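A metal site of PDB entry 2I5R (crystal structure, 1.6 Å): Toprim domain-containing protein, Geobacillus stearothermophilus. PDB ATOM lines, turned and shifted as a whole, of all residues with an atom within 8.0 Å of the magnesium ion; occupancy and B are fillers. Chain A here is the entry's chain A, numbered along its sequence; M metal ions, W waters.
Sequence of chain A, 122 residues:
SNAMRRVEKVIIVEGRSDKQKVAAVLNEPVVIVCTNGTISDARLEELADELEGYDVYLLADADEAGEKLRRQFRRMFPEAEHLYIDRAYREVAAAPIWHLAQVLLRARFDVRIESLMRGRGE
The side-chain carboxylate (OD1) of Asp 63 sits at hydrogen-bond distance from the backbone NH (N) of Gly 66 (2.9 Å).
The backbone NH (N) of Val 92 lies within hydrogen-bond range of the side-chain carboxylate (OD1) of Asp 61.
The magnesium ion is bound by water W1 (2.0 Å), water W2 (2.0 Å), the side-chain carboxylate (OD2) of Asp 61 (2.1 Å), the side-chain carboxylate (OE2) of Glu 91 (2.1 Å), the side-chain carboxylate (OD2) of Asp 63 (2.1 Å) and water W3 (2.2 Å).
The magnesium ion has six donor atoms within binding distance.
Within 4 Å of the magnesium ion: Asp 61, Asp 63 and Glu 91.
Water W2 lies within hydrogen-bond range of the side-chain carboxylate (OD1) of Asp 63 (2.6 Å) and the side-chain carboxylate (OE1) of Glu 14 (2.7 Å).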
ATOM      1  N   GLU A  14      20.309   6.244  30.480  1.00  0.00           N
ATOM      2  CA  GLU A  14      20.977   7.550  30.496  1.00  0.00           C
ATOM      3  C   GLU A  14      20.325   8.523  31.479  1.00  0.00           C
ATOM      4  O   GLU A  14      21.040   9.288  32.154  1.00  0.00           O
ATOM      5  CB  GLU A  14      20.987   8.167  29.077  1.00  0.00           C
ATOM      6  CG  GLU A  14      21.921   9.400  28.930  1.00  0.00           C
ATOM      7  CD  GLU A  14      21.745  10.156  27.620  1.00  0.00           C
ATOM      8  OE1 GLU A  14      20.840   9.792  26.815  1.00  0.00           O
ATOM      9  OE2 GLU A  14      22.501  11.124  27.403  1.00  0.00           O
ATOM     10  N   ASP A  18      14.057   7.863  31.849  1.00  0.00           N
ATOM     11  CA  ASP A  18      14.229   6.539  31.241  1.00  0.00           C
ATOM     12  C   ASP A  18      14.097   5.458  32.312  1.00  0.00           C
ATOM     13  O   ASP A  18      13.470   4.423  32.104  1.00  0.00           O
ATOM     14  CB  ASP A  18      15.595   6.370  30.562  1.00  0.00           C
ATOM     15  CG  ASP A  18      15.794   7.311  29.363  1.00  0.00           C
ATOM     16  OD1 ASP A  18      14.823   7.968  28.923  1.00  0.00           O
ATOM     17  OD2 ASP A  18      16.958   7.387  28.881  1.00  0.00           O
ATOM     18  N   ALA A  60      19.739   2.619  25.484  1.00  0.00           N
ATOM     19  CA  ALA A  60      20.029   4.034  25.189  1.00  0.00           C
ATOM     20  C   ALA A  60      19.135   4.562  24.066  1.00  0.00           C
ATOM     21  O   ALA A  60      18.607   3.783  23.242  1.00  0.00           O
ATOM     22  CB  ALA A  60      21.512   4.205  24.803  1.00  0.00           C
ATOM     23  N   ASP A  61      19.007   5.887  23.983  1.00  0.00           N
ATOM     24  CA  ASP A  61      18.224   6.513  22.920  1.00  0.00           C
ATOM     25  C   ASP A  61      18.823   6.257  21.548  1.00  0.00           C
ATOM     26  O   ASP A  61      20.021   6.000  21.453  1.00  0.00           O
ATOM     27  CB  ASP A  61      18.170   8.034  23.093  1.00  0.00           C
ATOM     28  CG  ASP A  61      17.360   8.489  24.299  1.00  0.00           C
ATOM     29  OD1 ASP A  61      16.628   7.705  24.933  1.00  0.00           O
ATOM     30  OD2 ASP A  61      17.457   9.712  24.579  1.00  0.00           O
ATOM     31  N   ALA A  62      17.991   6.343  20.506  1.00  0.00           N
ATOM     32  CA  ALA A  62      18.450   6.412  19.108  1.00  0.00           C
ATOM     33  C   ALA A  62      18.839   7.839  18.720  1.00  0.00           C
ATOM     34  O   ALA A  62      18.146   8.503  17.937  1.00  0.00           O
ATOM     35  CB  ALA A  62      17.376   5.874  18.150  1.00  0.00           C
ATOM     36  N   ASP A  63      19.931   8.338  19.301  1.00  0.00           N
ATOM     37  CA  ASP A  63      20.423   9.663  18.985  1.00  0.00           C
ATOM     38  C   ASP A  63      21.916   9.694  19.233  1.00  0.00           C
ATOM     39  O   ASP A  63      22.458   8.686  19.708  1.00  0.00           O
ATOM     40  CB  ASP A  63      19.627  10.766  19.747  1.00  0.00           C
ATOM     41  CG  ASP A  63      19.558  10.534  21.242  1.00  0.00           C
ATOM     42  OD1 ASP A  63      20.464   9.910  21.821  1.00  0.00           O
ATOM     43  OD2 ASP A  63      18.573  11.016  21.866  1.00  0.00           O
ATOM     44  N   GLU A  64      22.579  10.814  18.938  1.00  0.00           N
ATOM     45  CA  GLU A  64      24.033  10.884  19.082  1.00  0.00           C
ATOM     46  C   GLU A  64      24.527  10.647  20.514  1.00  0.00           C
ATOM     47  O   GLU A  64      25.536   9.952  20.718  1.00  0.00           O
ATOM     48  CB  GLU A  64      24.601  12.181  18.484  1.00  0.00           C
ATOM     49  CG  GLU A  64      24.456  13.426  19.342  1.00  0.00           C
ATOM     50  CD  GLU A  64      24.962  14.685  18.633  1.00  0.00           C
ATOM     51  OE1 GLU A  64      24.276  15.721  18.716  1.00  0.00           O
ATOM     52  OE2 GLU A  64      26.035  14.629  17.980  1.00  0.00           O
ATOM     53  N   ALA A  65      23.810  11.189  21.496  1.00  0.00           N
ATOM     54  CA  ALA A  65      24.212  11.044  22.889  1.00  0.00           C
ATOM     55  C   ALA A  65      24.058   9.586  23.304  1.00  0.00           C
ATOM     56  O   ALA A  65      24.925   9.049  24.035  1.00  0.00           O
ATOM     57  CB  ALA A  65      23.390  11.951  23.787  1.00  0.00           C
ATOM     58  N   GLY A  66      22.983   8.940  22.859  1.00  0.00           N
ATOM     59  CA  GLY A  66      22.763   7.514  23.185  1.00  0.00           C
ATOM     60  C   GLY A  66      23.861   6.673  22.569  1.00  0.00           C
ATOM     61  O   GLY A  66      24.417   5.778  23.199  1.00  0.00           O
ATOM     62  N   GLU A  67      24.207   6.989  21.314  1.00  0.00           N
ATOM     63  CA  GLU A  67      25.265   6.276  20.626  1.00  0.00           C
ATOM     64  C   GLU A  67      26.650   6.477  21.259  1.00  0.00           C
ATOM     65  O   GLU A  67      27.452   5.533  21.292  1.00  0.00           O
ATOM     66  CB  GLU A  67      25.277   6.650  19.146  1.00  0.00           C
ATOM     67  CG  GLU A  67      26.415   6.014  18.369  1.00  0.00           C
ATOM     68  CD  GLU A  67      26.388   4.501  18.389  1.00  0.00           C
ATOM     69  OE1 GLU A  67      25.364   3.895  18.789  1.00  0.00           O
ATOM     70  OE2 GLU A  67      27.402   3.900  17.981  1.00  0.00           O
ATOM     71  N   ARG A  90      12.648   7.138  18.630  1.00  0.00           N
ATOM     72  CA  ARG A  90      13.837   7.973  18.809  1.00  0.00           C
ATOM     73  C   ARG A  90      14.407   7.872  20.211  1.00  0.00           C
ATOM     74  O   ARG A  90      15.564   7.480  20.380  1.00  0.00           O
ATOM     75  CB  ARG A  90      13.561   9.443  18.494  1.00  0.00           C
ATOM     76  CG  ARG A  90      14.771  10.334  18.673  1.00  0.00           C
ATOM     77  CD  ARG A  90      15.228  10.957  17.364  1.00  0.00           C
ATOM     78  NE  ARG A  90      16.531  11.611  17.547  1.00  0.00           N
ATOM     79  CZ  ARG A  90      17.285  12.076  16.560  1.00  0.00           C
ATOM     80  NH1 ARG A  90      16.880  11.968  15.307  1.00  0.00           N
ATOM     81  NH2 ARG A  90      18.449  12.662  16.842  1.00  0.00           N
ATOM     82  N   GLU A  91      13.600   8.238  21.209  1.00  0.00           N
ATOM     83  CA  GLU A  91      14.082   8.218  22.591  1.00  0.00           C
ATOM     84  C   GLU A  91      13.275   7.295  23.476  1.00  0.00           C
ATOM     85  O   GLU A  91      12.068   7.114  23.289  1.00  0.00           O
ATOM     86  CB  GLU A  91      14.149   9.630  23.162  1.00  0.00           C
ATOM     87  CG  GLU A  91      15.108  10.538  22.410  1.00  0.00           C
ATOM     88  CD  GLU A  91      15.309  11.862  23.127  1.00  0.00           C
ATOM     89  OE1 GLU A  91      14.274  12.529  23.348  1.00  0.00           O
ATOM     90  OE2 GLU A  91      16.475  12.230  23.461  1.00  0.00           O
ATOM     91  N   VAL A  92      13.947   6.681  24.439  1.00  0.00           N
ATOM     92  CA  VAL A  92      13.279   5.817  25.408  1.00  0.00           C
ATOM     93  C   VAL A  92      12.088   6.553  26.032  1.00  0.00           C
ATOM     94  O   VAL A  92      11.010   5.983  26.201  1.00  0.00           O
ATOM     95  CB  VAL A  92      14.272   5.322  26.513  1.00  0.00           C
ATOM     96  CG1 VAL A  92      13.549   4.501  27.583  1.00  0.00           C
ATOM     97  CG2 VAL A  92      15.399   4.531  25.887  1.00  0.00           C
ATOM     98  N   ALA A  93      12.288   7.834  26.340  1.00  0.00           N
ATOM     99  CA  ALA A  93      11.234   8.662  26.928  1.00  0.00           C
ATOM    100  C   ALA A  93       9.996   8.791  26.034  1.00  0.00           C
ATOM    101  O   ALA A  93       8.871   8.911  26.538  1.00  0.00           O
ATOM    102  CB  ALA A  93      11.781  10.034  27.287  1.00  0.00           C
HETATM  103 MG    MG M   1      18.377  11.471  23.925  1.00  0.00          MG
HETATM  104  O   HOH W   1      19.370  13.166  23.496  1.00  0.00           O
HETATM  105  O   HOH W   2      20.174  10.619  24.351  1.00  0.00           O
HETATM  106  O   HOH W   3      18.125  12.171  25.965  1.00  0.00           O
